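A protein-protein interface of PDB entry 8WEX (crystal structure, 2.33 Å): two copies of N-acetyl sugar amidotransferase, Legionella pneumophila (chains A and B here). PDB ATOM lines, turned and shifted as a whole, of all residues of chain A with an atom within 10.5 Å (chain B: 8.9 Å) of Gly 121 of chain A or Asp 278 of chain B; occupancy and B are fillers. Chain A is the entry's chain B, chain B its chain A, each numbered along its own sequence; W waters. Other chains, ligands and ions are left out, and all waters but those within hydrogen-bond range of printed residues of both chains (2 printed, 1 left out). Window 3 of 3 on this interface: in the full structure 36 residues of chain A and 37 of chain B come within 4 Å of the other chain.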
ATOM      1  N   PHE A 116     -31.375  21.910  21.673  1.00  0.00           N
ATOM      2  CA  PHE A 116     -31.033  21.177  20.421  1.00  0.00           C
ATOM      3  C   PHE A 116     -31.149  19.659  20.589  1.00  0.00           C
ATOM      4  O   PHE A 116     -31.271  18.966  19.564  1.00  0.00           O
ATOM      5  CB  PHE A 116     -29.630  21.539  19.926  1.00  0.00           C
ATOM      6  CG  PHE A 116     -29.575  22.864  19.221  1.00  0.00           C
ATOM      7  CD1 PHE A 116     -30.093  23.013  17.946  1.00  0.00           C
ATOM      8  CD2 PHE A 116     -29.035  23.970  19.855  1.00  0.00           C
ATOM      9  CE1 PHE A 116     -30.063  24.247  17.320  1.00  0.00           C
ATOM     10  CE2 PHE A 116     -28.979  25.195  19.214  1.00  0.00           C
ATOM     11  CZ  PHE A 116     -29.507  25.336  17.954  1.00  0.00           C
ATOM     12  N   ARG A 117     -31.100  19.137  21.814  1.00  0.00           N
ATOM     13  CA  ARG A 117     -31.093  17.670  22.037  1.00  0.00           C
ATOM     14  C   ARG A 117     -32.224  17.036  21.221  1.00  0.00           C
ATOM     15  O   ARG A 117     -33.349  17.576  21.226  1.00  0.00           O
ATOM     16  CB  ARG A 117     -31.225  17.328  23.521  1.00  0.00           C
ATOM     17  CG  ARG A 117     -31.026  15.850  23.830  1.00  0.00           C
ATOM     18  CD  ARG A 117     -30.691  15.580  25.288  1.00  0.00           C
ATOM     19  NE  ARG A 117     -31.059  16.700  26.145  1.00  0.00           N
ATOM     20  CZ  ARG A 117     -30.207  17.522  26.745  1.00  0.00           C
ATOM     21  NH1 ARG A 117     -28.906  17.363  26.610  1.00  0.00           N
ATOM     22  NH2 ARG A 117     -30.670  18.514  27.481  1.00  0.00           N
ATOM     23  N   SER A 118     -31.920  15.932  20.542  1.00  0.00           N
ATOM     24  CA  SER A 118     -32.849  15.173  19.672  1.00  0.00           C
ATOM     25  C   SER A 118     -33.604  14.143  20.517  1.00  0.00           C
ATOM     26  O   SER A 118     -32.954  13.417  21.301  1.00  0.00           O
ATOM     27  CB  SER A 118     -32.107  14.505  18.545  1.00  0.00           C
ATOM     28  OG  SER A 118     -32.720  13.273  18.174  1.00  0.00           O
ATOM     29  N   LYS A 119     -34.925  14.075  20.351  1.00  0.00           N
ATOM     30  CA  LYS A 119     -35.799  13.145  21.115  1.00  0.00           C
ATOM     31  C   LYS A 119     -35.931  11.822  20.358  1.00  0.00           C
ATOM     32  O   LYS A 119     -36.071  10.786  21.009  1.00  0.00           O
ATOM     33  CB  LYS A 119     -37.183  13.760  21.347  1.00  0.00           C
ATOM     34  CG  LYS A 119     -37.273  14.778  22.473  1.00  0.00           C
ATOM     35  CD  LYS A 119     -38.531  14.636  23.306  1.00  0.00           C
ATOM     36  CE  LYS A 119     -39.059  15.961  23.809  1.00  0.00           C
ATOM     37  NZ  LYS A 119     -40.291  15.772  24.609  1.00  0.00           N
ATOM     38  N   ASP A 120     -35.887  11.871  19.024  1.00  0.00           N
ATOM     39  CA  ASP A 120     -35.842  10.698  18.117  1.00  0.00           C
ATOM     40  C   ASP A 120     -34.417  10.132  18.131  1.00  0.00           C
ATOM     41  O   ASP A 120     -33.659  10.451  19.077  1.00  0.00           O
ATOM     42  CB  ASP A 120     -36.301  11.070  16.700  1.00  0.00           C
ATOM     43  CG  ASP A 120     -35.706  12.352  16.128  1.00  0.00           C
ATOM     44  OD1 ASP A 120     -35.246  13.196  16.909  1.00  0.00           O
ATOM     45  OD2 ASP A 120     -35.725  12.507  14.902  1.00  0.00           O
ATOM     46  N   GLY A 121     -34.065   9.318  17.132  1.00  0.00           N
ATOM     47  CA  GLY A 121     -32.736   8.688  17.036  1.00  0.00           C
ATOM     48  C   GLY A 121     -31.816   9.441  16.097  1.00  0.00           C
ATOM     49  O   GLY A 121     -30.863   8.814  15.586  1.00  0.00           O
ATOM     50  N   SER A 122     -32.085  10.720  15.835  1.00  0.00           N
ATOM     51  CA  SER A 122     -31.277  11.509  14.871  1.00  0.00           C
ATOM     52  C   SER A 122     -30.143  12.229  15.611  1.00  0.00           C
ATOM     53  O   SER A 122     -30.221  12.428  16.837  1.00  0.00           O
ATOM     54  CB  SER A 122     -32.117  12.467  14.075  1.00  0.00           C
ATOM     55  OG  SER A 122     -32.748  13.391  14.942  1.00  0.00           O
ATOM     56  N   TYR A 123     -29.107  12.591  14.870  1.00  0.00           N
ATOM     57  CA  TYR A 123     -28.003  13.435  15.384  1.00  0.00           C
ATOM     58  C   TYR A 123     -28.592  14.782  15.756  1.00  0.00           C
ATOM     59  O   TYR A 123     -29.435  15.286  15.002  1.00  0.00           O
ATOM     60  CB  TYR A 123     -26.899  13.622  14.348  1.00  0.00           C
ATOM     61  CG  TYR A 123     -26.260  12.339  13.884  1.00  0.00           C
ATOM     62  CD1 TYR A 123     -25.553  11.523  14.753  1.00  0.00           C
ATOM     63  CD2 TYR A 123     -26.344  11.953  12.562  1.00  0.00           C
ATOM     64  CE1 TYR A 123     -24.949  10.355  14.316  1.00  0.00           C
ATOM     65  CE2 TYR A 123     -25.753  10.788  12.107  1.00  0.00           C
ATOM     66  CZ  TYR A 123     -25.058   9.983  12.986  1.00  0.00           C
ATOM     67  OH  TYR A 123     -24.480   8.841  12.510  1.00  0.00           O
ATOM     68  N   ASP A 124     -28.145  15.348  16.871  1.00  0.00           N
ATOM     69  CA  ASP A 124     -28.551  16.710  17.307  1.00  0.00           C
ATOM     70  C   ASP A 124     -27.349  17.664  17.267  1.00  0.00           C
ATOM     71  O   ASP A 124     -27.467  18.800  17.721  1.00  0.00           O
ATOM     72  CB  ASP A 124     -29.164  16.656  18.702  1.00  0.00           C
ATOM     73  CG  ASP A 124     -28.384  15.800  19.682  1.00  0.00           C
ATOM     74  OD1 ASP A 124     -27.135  15.826  19.597  1.00  0.00           O
ATOM     75  OD2 ASP A 124     -29.028  15.100  20.513  1.00  0.00           O
ATOM     76  N   CYS A 125     -26.214  17.236  16.740  1.00  0.00           N
ATOM     77  CA  CYS A 125     -24.920  17.900  17.031  1.00  0.00           C
ATOM     78  C   CYS A 125     -23.863  17.454  16.010  1.00  0.00           C
ATOM     79  O   CYS A 125     -23.807  16.257  15.703  1.00  0.00           O
ATOM     80  CB  CYS A 125     -24.595  17.563  18.485  1.00  0.00           C
ATOM     81  SG  CYS A 125     -23.038  18.225  19.082  1.00  0.00           S
ATOM     82  N   LYS A 143     -21.573  13.980  24.635  1.00  0.00           N
ATOM     83  CA  LYS A 143     -22.374  12.739  24.587  1.00  0.00           C
ATOM     84  C   LYS A 143     -22.616  12.242  26.016  1.00  0.00           C
ATOM     85  O   LYS A 143     -23.793  12.054  26.376  1.00  0.00           O
ATOM     86  CB  LYS A 143     -21.702  11.672  23.721  1.00  0.00           C
ATOM     87  CG  LYS A 143     -22.463  10.357  23.636  1.00  0.00           C
ATOM     88  CD  LYS A 143     -21.934   9.414  22.601  1.00  0.00           C
ATOM     89  CE  LYS A 143     -22.811   8.197  22.441  1.00  0.00           C
ATOM     90  NZ  LYS A 143     -22.573   7.531  21.135  1.00  0.00           N
ATOM     91  N   MET A 148     -25.924  14.466  24.581  1.00  0.00           N
ATOM     92  CA  MET A 148     -26.079  14.834  23.156  1.00  0.00           C
ATOM     93  C   MET A 148     -25.787  13.601  22.311  1.00  0.00           C
ATOM     94  O   MET A 148     -25.308  12.601  22.862  1.00  0.00           O
ATOM     95  CB  MET A 148     -25.142  15.985  22.770  1.00  0.00           C
ATOM     96  CG  MET A 148     -25.432  17.254  23.539  1.00  0.00           C
ATOM     97  SD  MET A 148     -27.188  17.742  23.454  1.00  0.00           S
ATOM     98  CE  MET A 148     -27.175  18.756  21.980  1.00  0.00           C
ATOM     99  N   ASN A 149     -26.092  13.693  21.022  1.00  0.00           N
ATOM    100  CA  ASN A 149     -25.880  12.624  20.017  1.00  0.00           C
ATOM    101  C   ASN A 149     -25.093  13.242  18.872  1.00  0.00           C
ATOM    102  O   ASN A 149     -25.643  13.539  17.813  1.00  0.00           O
ATOM    103  CB  ASN A 149     -27.200  12.010  19.555  1.00  0.00           C
ATOM    104  CG  ASN A 149     -28.036  11.501  20.711  1.00  0.00           C
ATOM    105  OD1 ASN A 149     -27.942  10.327  21.079  1.00  0.00           O
ATOM    106  ND2 ASN A 149     -28.836  12.383  21.301  1.00  0.00           N
ATOM    107  N   PRO A 150     -23.792  13.515  19.074  1.00  0.00           N
ATOM    108  CA  PRO A 150     -22.991  14.117  18.017  1.00  0.00           C
ATOM    109  C   PRO A 150     -22.644  13.096  16.930  1.00  0.00           C
ATOM    110  O   PRO A 150     -22.321  11.949  17.230  1.00  0.00           O
ATOM    111  CB  PRO A 150     -21.737  14.590  18.743  1.00  0.00           C
ATOM    112  CG  PRO A 150     -21.608  13.643  19.911  1.00  0.00           C
ATOM    113  CD  PRO A 150     -23.015  13.232  20.292  1.00  0.00           C
ATOM    114  N   LEU A 151     -22.745  13.539  15.688  1.00  0.00           N
ATOM    115  CA  LEU A 151     -21.970  12.972  14.563  1.00  0.00           C
ATOM    116  C   LEU A 151     -20.621  13.691  14.530  1.00  0.00           C
ATOM    117  O   LEU A 151     -20.594  14.914  14.535  1.00  0.00           O
ATOM    118  CB  LEU A 151     -22.721  13.179  13.248  1.00  0.00           C
ATOM    119  CG  LEU A 151     -21.904  12.871  11.996  1.00  0.00           C
ATOM    120  CD1 LEU A 151     -21.588  11.388  11.908  1.00  0.00           C
ATOM    121  CD2 LEU A 151     -22.634  13.349  10.757  1.00  0.00           C
ATOM    122  N   ASP A 177     -20.037   7.847  15.650  1.00  0.00           N
ATOM    123  CA  ASP A 177     -20.073   7.808  14.178  1.00  0.00           C
ATOM    124  C   ASP A 177     -19.146   8.925  13.692  1.00  0.00           C
ATOM    125  O   ASP A 177     -19.016   9.964  14.371  1.00  0.00           O
ATOM    126  CB  ASP A 177     -21.502   7.956  13.671  1.00  0.00           C
ATOM    127  CG  ASP A 177     -22.427   6.782  13.995  1.00  0.00           C
ATOM    128  OD1 ASP A 177     -21.942   5.664  14.275  1.00  0.00           O
ATOM    129  OD2 ASP A 177     -23.636   6.999  13.957  1.00  0.00           O
ATOM    130  N   HIS A 221     -26.391  16.553   6.512  1.00  0.00           N
ATOM    131  CA  HIS A 221     -27.089  15.668   7.479  1.00  0.00           C
ATOM    132  C   HIS A 221     -28.288  16.385   8.109  1.00  0.00           C
ATOM    133  O   HIS A 221     -28.939  15.760   8.961  1.00  0.00           O
ATOM    134  CB  HIS A 221     -26.113  15.155   8.536  1.00  0.00           C
ATOM    135  CG  HIS A 221     -25.050  14.272   7.982  1.00  0.00           C
ATOM    136  ND1 HIS A 221     -25.242  12.920   7.745  1.00  0.00           N
ATOM    137  CD2 HIS A 221     -23.780  14.545   7.612  1.00  0.00           C
ATOM    138  CE1 HIS A 221     -24.129  12.405   7.252  1.00  0.00           C
ATOM    139  NE2 HIS A 221     -23.214  13.383   7.158  1.00  0.00           N
ATOM    140  N   ILE A 223     -28.371  18.836  10.224  1.00  0.00           N
ATOM    141  CA  ILE A 223     -28.118  19.094  11.667  1.00  0.00           C
ATOM    142  C   ILE A 223     -27.947  20.599  11.819  1.00  0.00           C
ATOM    143  O   ILE A 223     -27.359  21.207  10.942  1.00  0.00           O
ATOM    144  CB  ILE A 223     -26.894  18.307  12.161  1.00  0.00           C
ATOM    145  CG1 ILE A 223     -27.103  16.801  11.995  1.00  0.00           C
ATOM    146  CG2 ILE A 223     -26.565  18.670  13.607  1.00  0.00           C
ATOM    147  CD1 ILE A 223     -25.827  15.989  11.949  1.00  0.00           C
ATOM    148  N   VAL B 187     -20.561   0.349  19.312  1.00  0.00           N
ATOM    149  CA  VAL B 187     -21.799  -0.265  18.759  1.00  0.00           C
ATOM    150  C   VAL B 187     -21.400  -1.335  17.747  1.00  0.00           C
ATOM    151  O   VAL B 187     -21.980  -2.417  17.760  1.00  0.00           O
ATOM    152  CB  VAL B 187     -22.725   0.800  18.147  1.00  0.00           C
ATOM    153  CG1 VAL B 187     -23.821   0.195  17.303  1.00  0.00           C
ATOM    154  CG2 VAL B 187     -23.309   1.685  19.230  1.00  0.00           C
ATOM    155  N   LYS B 257     -40.526  -3.049  17.945  1.00  0.00           N
ATOM    156  CA  LYS B 257     -39.048  -3.193  18.040  1.00  0.00           C
ATOM    157  C   LYS B 257     -38.646  -4.674  18.142  1.00  0.00           C
ATOM    158  O   LYS B 257     -37.485  -4.967  17.779  1.00  0.00           O
ATOM    159  CB  LYS B 257     -38.505  -2.391  19.228  1.00  0.00           C
ATOM    160  N   ILE B 260     -37.727  -6.368  14.364  1.00  0.00           N
ATOM    161  CA  ILE B 260     -36.477  -6.069  13.592  1.00  0.00           C
ATOM    162  C   ILE B 260     -35.273  -6.625  14.357  1.00  0.00           C
ATOM    163  O   ILE B 260     -35.274  -6.559  15.599  1.00  0.00           O
ATOM    164  CB  ILE B 260     -36.316  -4.564  13.298  1.00  0.00           C
ATOM    165  CG1 ILE B 260     -37.652  -3.905  12.942  1.00  0.00           C
ATOM    166  CG2 ILE B 260     -35.264  -4.325  12.218  1.00  0.00           C
ATOM    167  CD1 ILE B 260     -38.298  -3.152  14.085  1.00  0.00           C
ATOM    168  N   VAL B 267     -34.029  -5.143  18.019  1.00  0.00           N
ATOM    169  CA  VAL B 267     -33.803  -3.726  18.397  1.00  0.00           C
ATOM    170  C   VAL B 267     -34.319  -3.545  19.826  1.00  0.00           C
ATOM    171  O   VAL B 267     -33.606  -2.906  20.629  1.00  0.00           O
ATOM    172  CB  VAL B 267     -34.492  -2.758  17.421  1.00  0.00           C
ATOM    173  CG1 VAL B 267     -34.136  -1.322  17.755  1.00  0.00           C
ATOM    174  CG2 VAL B 267     -34.140  -3.068  15.977  1.00  0.00           C
ATOM    175  N   GLN B 268     -35.494  -4.107  20.130  1.00  0.00           N
ATOM    176  CA  GLN B 268     -36.137  -4.001  21.467  1.00  0.00           C
ATOM    177  C   GLN B 268     -35.137  -4.447  22.539  1.00  0.00           C
ATOM    178  O   GLN B 268     -34.956  -3.677  23.505  1.00  0.00           O
ATOM    179  CB  GLN B 268     -37.428  -4.818  21.542  1.00  0.00           C
ATOM    180  CG  GLN B 268     -38.152  -4.678  22.881  1.00  0.00           C
ATOM    181  CD  GLN B 268     -39.617  -5.044  22.809  1.00  0.00           C
ATOM    182  OE1 GLN B 268     -39.988  -6.202  22.626  1.00  0.00           O
ATOM    183  NE2 GLN B 268     -40.476  -4.046  22.952  1.00  0.00           N
ATOM    184  N   LEU B 270     -31.807  -4.925  22.131  1.00  0.00           N
ATOM    185  CA  LEU B 270     -30.569  -4.113  22.040  1.00  0.00           C
ATOM    186  C   LEU B 270     -30.700  -2.911  22.983  1.00  0.00           C
ATOM    187  O   LEU B 270     -29.783  -2.675  23.795  1.00  0.00           O
ATOM    188  CB  LEU B 270     -30.331  -3.670  20.594  1.00  0.00           C
ATOM    189  CG  LEU B 270     -29.763  -4.745  19.673  1.00  0.00           C
ATOM    190  CD1 LEU B 270     -29.721  -4.253  18.241  1.00  0.00           C
ATOM    191  CD2 LEU B 270     -28.384  -5.195  20.141  1.00  0.00           C
ATOM    192  N   LYS B 271     -31.833  -2.211  22.914  1.00  0.00           N
ATOM    193  CA  LYS B 271     -32.090  -1.006  23.737  1.00  0.00           C
ATOM    194  C   LYS B 271     -32.376  -1.417  25.185  1.00  0.00           C
ATOM    195  O   LYS B 271     -31.719  -0.874  26.111  1.00  0.00           O
ATOM    196  CB  LYS B 271     -33.246  -0.210  23.136  1.00  0.00           C
ATOM    197  CG  LYS B 271     -33.092   0.111  21.650  1.00  0.00           C
ATOM    198  CD  LYS B 271     -34.360   0.594  20.996  1.00  0.00           C
ATOM    199  CE  LYS B 271     -34.890   1.847  21.657  1.00  0.00           C
ATOM    200  NZ  LYS B 271     -36.138   2.318  21.021  1.00  0.00           N
ATOM    201  N   GLY B 275     -28.017  -1.529  26.250  1.00  0.00           N
ATOM    202  CA  GLY B 275     -27.645  -0.128  26.525  1.00  0.00           C
ATOM    203  C   GLY B 275     -27.530   0.692  25.253  1.00  0.00           C
ATOM    204  O   GLY B 275     -26.773   1.677  25.257  1.00  0.00           O
ATOM    205  N   LEU B 276     -28.253   0.311  24.201  1.00  0.00           N
ATOM    206  CA  LEU B 276     -28.269   1.071  22.927  1.00  0.00           C
ATOM    207  C   LEU B 276     -29.507   1.960  22.885  1.00  0.00           C
ATOM    208  O   LEU B 276     -30.492   1.652  23.572  1.00  0.00           O
ATOM    209  CB  LEU B 276     -28.244   0.114  21.735  1.00  0.00           C
ATOM    210  CG  LEU B 276     -26.988  -0.742  21.598  1.00  0.00           C
ATOM    211  CD1 LEU B 276     -26.961  -1.407  20.228  1.00  0.00           C
ATOM    212  CD2 LEU B 276     -25.727   0.083  21.829  1.00  0.00           C
ATOM    213  N   ASN B 277     -29.428   3.026  22.092  1.00  0.00           N
ATOM    214  CA  ASN B 277     -30.560   3.935  21.799  1.00  0.00           C
ATOM    215  C   ASN B 277     -30.761   3.934  20.288  1.00  0.00           C
ATOM    216  O   ASN B 277     -29.996   3.246  19.591  1.00  0.00           O
ATOM    217  CB  ASN B 277     -30.326   5.338  22.364  1.00  0.00           C
ATOM    218  CG  ASN B 277     -28.965   5.896  22.016  1.00  0.00           C
ATOM    219  OD1 ASN B 277     -28.588   5.944  20.851  1.00  0.00           O
ATOM    220  ND2 ASN B 277     -28.208   6.296  23.023  1.00  0.00           N
ATOM    221  N   ASP B 278     -31.755   4.679  19.814  1.00  0.00           N
ATOM    222  CA  ASP B 278     -32.142   4.705  18.382  1.00  0.00           C
ATOM    223  C   ASP B 278     -31.029   5.360  17.570  1.00  0.00           C
ATOM    224  O   ASP B 278     -30.845   4.950  16.414  1.00  0.00           O
ATOM    225  CB  ASP B 278     -33.477   5.418  18.176  1.00  0.00           C
ATOM    226  CG  ASP B 278     -34.676   4.601  18.617  1.00  0.00           C
ATOM    227  OD1 ASP B 278     -34.573   3.353  18.605  1.00  0.00           O
ATOM    228  OD2 ASP B 278     -35.693   5.217  18.987  1.00  0.00           O
ATOM    229  N   ASN B 279     -30.328   6.338  18.149  1.00  0.00           N
ATOM    230  CA  ASN B 279     -29.227   7.060  17.461  1.00  0.00           C
ATOM    231  C   ASN B 279     -28.096   6.069  17.162  1.00  0.00           C
ATOM    232  O   ASN B 279     -27.576   6.121  16.030  1.00  0.00           O
ATOM    233  CB  ASN B 279     -28.719   8.272  18.251  1.00  0.00           C
ATOM    234  CG  ASN B 279     -27.619   9.034  17.528  1.00  0.00           C
ATOM    235  OD1 ASN B 279     -26.515   9.207  18.058  1.00  0.00           O
ATOM    236  ND2 ASN B 279     -27.893   9.473  16.306  1.00  0.00           N
ATOM    237  N   ASP B 280     -27.750   5.188  18.111  1.00  0.00           N
ATOM    238  CA  ASP B 280     -26.681   4.169  17.932  1.00  0.00           C
ATOM    239  C   ASP B 280     -26.964   3.299  16.694  1.00  0.00           C
ATOM    240  O   ASP B 280     -25.996   2.771  16.089  1.00  0.00           O
ATOM    241  CB  ASP B 280     -26.539   3.324  19.194  1.00  0.00           C
ATOM    242  CG  ASP B 280     -26.043   4.083  20.417  1.00  0.00           C
ATOM    243  OD1 ASP B 280     -25.398   5.155  20.244  1.00  0.00           O
ATOM    244  OD2 ASP B 280     -26.322   3.601  21.548  1.00  0.00           O
ATOM    245  N   LEU B 281     -28.232   3.141  16.304  1.00  0.00           N
ATOM    246  CA  LEU B 281     -28.604   2.206  15.207  1.00  0.00           C
ATOM    247  C   LEU B 281     -29.012   2.979  13.952  1.00  0.00           C
ATOM    248  O   LEU B 281     -29.324   2.338  12.934  1.00  0.00           O
ATOM    249  CB  LEU B 281     -29.719   1.288  15.705  1.00  0.00           C
ATOM    250  CG  LEU B 281     -29.336   0.446  16.927  1.00  0.00           C
ATOM    251  CD1 LEU B 281     -30.541  -0.254  17.514  1.00  0.00           C
ATOM    252  CD2 LEU B 281     -28.255  -0.571  16.590  1.00  0.00           C
ATOM    253  N   ASP B 282     -28.981   4.310  14.009  1.00  0.00           N
ATOM    254  CA  ASP B 282     -29.446   5.171  12.896  1.00  0.00           C
ATOM    255  C   ASP B 282     -28.613   4.851  11.660  1.00  0.00           C
ATOM    256  O   ASP B 282     -29.170   4.840  10.559  1.00  0.00           O
ATOM    257  CB  ASP B 282     -29.374   6.647  13.279  1.00  0.00           C
ATOM    258  CG  ASP B 282     -29.989   7.566  12.241  1.00  0.00           C
ATOM    259  OD1 ASP B 282     -29.333   7.795  11.215  1.00  0.00           O
ATOM    260  OD2 ASP B 282     -31.130   8.023  12.463  1.00  0.00           O
ATOM    261  N   ALA B 283     -27.319   4.592  11.838  1.00  0.00           N
ATOM    262  CA  ALA B 283     -26.366   4.414  10.723  1.00  0.00           C
ATOM    263  C   ALA B 283     -26.718   3.152   9.924  1.00  0.00           C
ATOM    264  O   ALA B 283     -26.315   3.078   8.753  1.00  0.00           O
ATOM    265  CB  ALA B 283     -24.956   4.366  11.256  1.00  0.00           C
ATOM    266  N   TYR B 284     -27.436   2.200  10.527  1.00  0.00           N
ATOM    267  CA  TYR B 284     -27.747   0.888   9.904  1.00  0.00           C
ATOM    268  C   TYR B 284     -29.102   0.894   9.201  1.00  0.00           C
ATOM    269  O   TYR B 284     -29.373  -0.093   8.494  1.00  0.00           O
ATOM    270  CB  TYR B 284     -27.700  -0.215  10.955  1.00  0.00           C
ATOM    271  CG  TYR B 284     -26.336  -0.370  11.561  1.00  0.00           C
ATOM    272  CD1 TYR B 284     -25.399  -1.196  10.979  1.00  0.00           C
ATOM    273  CD2 TYR B 284     -25.973   0.337  12.693  1.00  0.00           C
ATOM    274  CE1 TYR B 284     -24.136  -1.345  11.526  1.00  0.00           C
ATOM    275  CE2 TYR B 284     -24.715   0.199  13.255  1.00  0.00           C
ATOM    276  CZ  TYR B 284     -23.795  -0.639  12.664  1.00  0.00           C
ATOM    277  OH  TYR B 284     -22.559  -0.725  13.219  1.00  0.00           O
ATOM    278  N   LEU B 285     -29.894   1.958   9.348  1.00  0.00           N
ATOM    279  CA  LEU B 285     -31.243   2.037   8.739  1.00  0.00           C
ATOM    280  C   LEU B 285     -31.111   2.100   7.224  1.00  0.00           C
ATOM    281  O   LEU B 285     -30.174   2.689   6.699  1.00  0.00           O
ATOM    282  CB  LEU B 285     -32.003   3.252   9.281  1.00  0.00           C
ATOM    283  CG  LEU B 285     -32.315   3.202  10.775  1.00  0.00           C
ATOM    284  CD1 LEU B 285     -33.433   4.175  11.115  1.00  0.00           C
ATOM    285  CD2 LEU B 285     -32.680   1.792  11.223  1.00  0.00           C
HETATM  286  O   HOH W   1     -24.550   7.433  16.812  1.00  0.00           O
HETATM  287  O   HOH W   2     -26.953   8.012  10.652  1.00  0.00           O
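The side-chain carboxylate (OD2) of Asp 177 of chain A sits at hydrogen-bond distance from the side-chain hydroxyl (OH) of Tyr 123 of chain A.
The backbone NH of Asp 280 of chain B lies within hydrogen-bond range of the side-chain amide oxygen of Asn 277 of chain B (3.0 Å).
The backbone NH (N) of Asn 149 of chain A is in hydrogen-bond range of the side-chain carboxylate (OD1) of Asp 124 of chain A, at 2.8 Å.
OG of Ser 122 of chain A is in hydrogen-bond range of OD2 of Asp 120 of chain A (3.1 Å).
The side-chain amino group of Lys 271 of chain B is in salt-bridge range of the side-chain carboxylate of Asp 278 of chain B, 3.1 Å away.
OD1 of Asn 277 of chain B sits at hydrogen-bond distance from N of Asn 279 of chain B, at 3.2 Å.
Water W2 bridges OD1 of Asp 282 of chain B (2.5 Å) and OH of Tyr 123 of chain A (3.2 Å).
Water W1 bridges OD1 of Asn 279 of chain B and OD2 of Asp 177 of chain A.
CB of Asp 278 of chain B touches CA of Gly 121 of chain A (3.5 Å).
Ser 122 of chain A touches Asn 279 of chain B (C to ND2, 3.6 Å).
ND2 of Asn 279 of chain B touches CD1 of Tyr 123 of chain A (3.5 Å).
Asn 279 of chain B touches Asn 149 of chain A (OD1 to CB, 3.3 Å).
Ala 283 of chain B touches Asp 177 of chain A.
Of the 18 printed residues of chain A, 6 touch a printed residue of chain B.
Among the printed residues, Asp or Glu carboxylates within 4 Å of a Lys or Arg side-chain nitrogen of the other chain: Lys 143 of chain A with Asp 280 of chain B.
O of Gly 121 of chain A lies close to ND2 of Asn 279 of chain B (3.1 Å).
The backbone carbonyl oxygen (O) of Gly 121 of chain A lies close to the side-chain carboxylate (OD2) of Asp 282 of chain B.
The side-chain carboxylate of Asp 280 of chain B lies within salt-bridge range of the side-chain amino group of Lys 143 of chain A (3.8 Å).
Of chain B, only Asp 278 (3.5 Å), Asn 279 (3.0 Å) and Asp 282 (3.2 Å) come within 4 Å of Gly 121 of chain A.
Of the printed residues of chain B, Tyr 123 of chain A touches Asn 279.
Of the printed residues of chain B, Asp 177 of chain A touches Ala 283.
No residue of chain A comes within 4 Å of Asn 277 of chain B.
Of chain A, only Gly 121 (3.5 Å) comes within 4 Å of Asp 278 of chain B.
Asn 279 of chain B touches just these residues of chain A: Gly 121, Ser 122, Tyr 123 and Asn 149.
Asp 280 of chain B touches one residue of chain A.
No residue of chain A comes within 4 Å of Leu 281 of chain B.
The nearest residue of chain A that does not touch Asp 278 of chain B is Asp 120 of chain A (4.8 Å).
The nearest printed residue of chain A that does not touch Ala 283 of chain B is Tyr 123 of chain A (4.7 Å).
No position is printed for both chains.
Of the 8 pairs that touch across the chains among the printed residues, none has its exchanged pair printed and touching as well.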
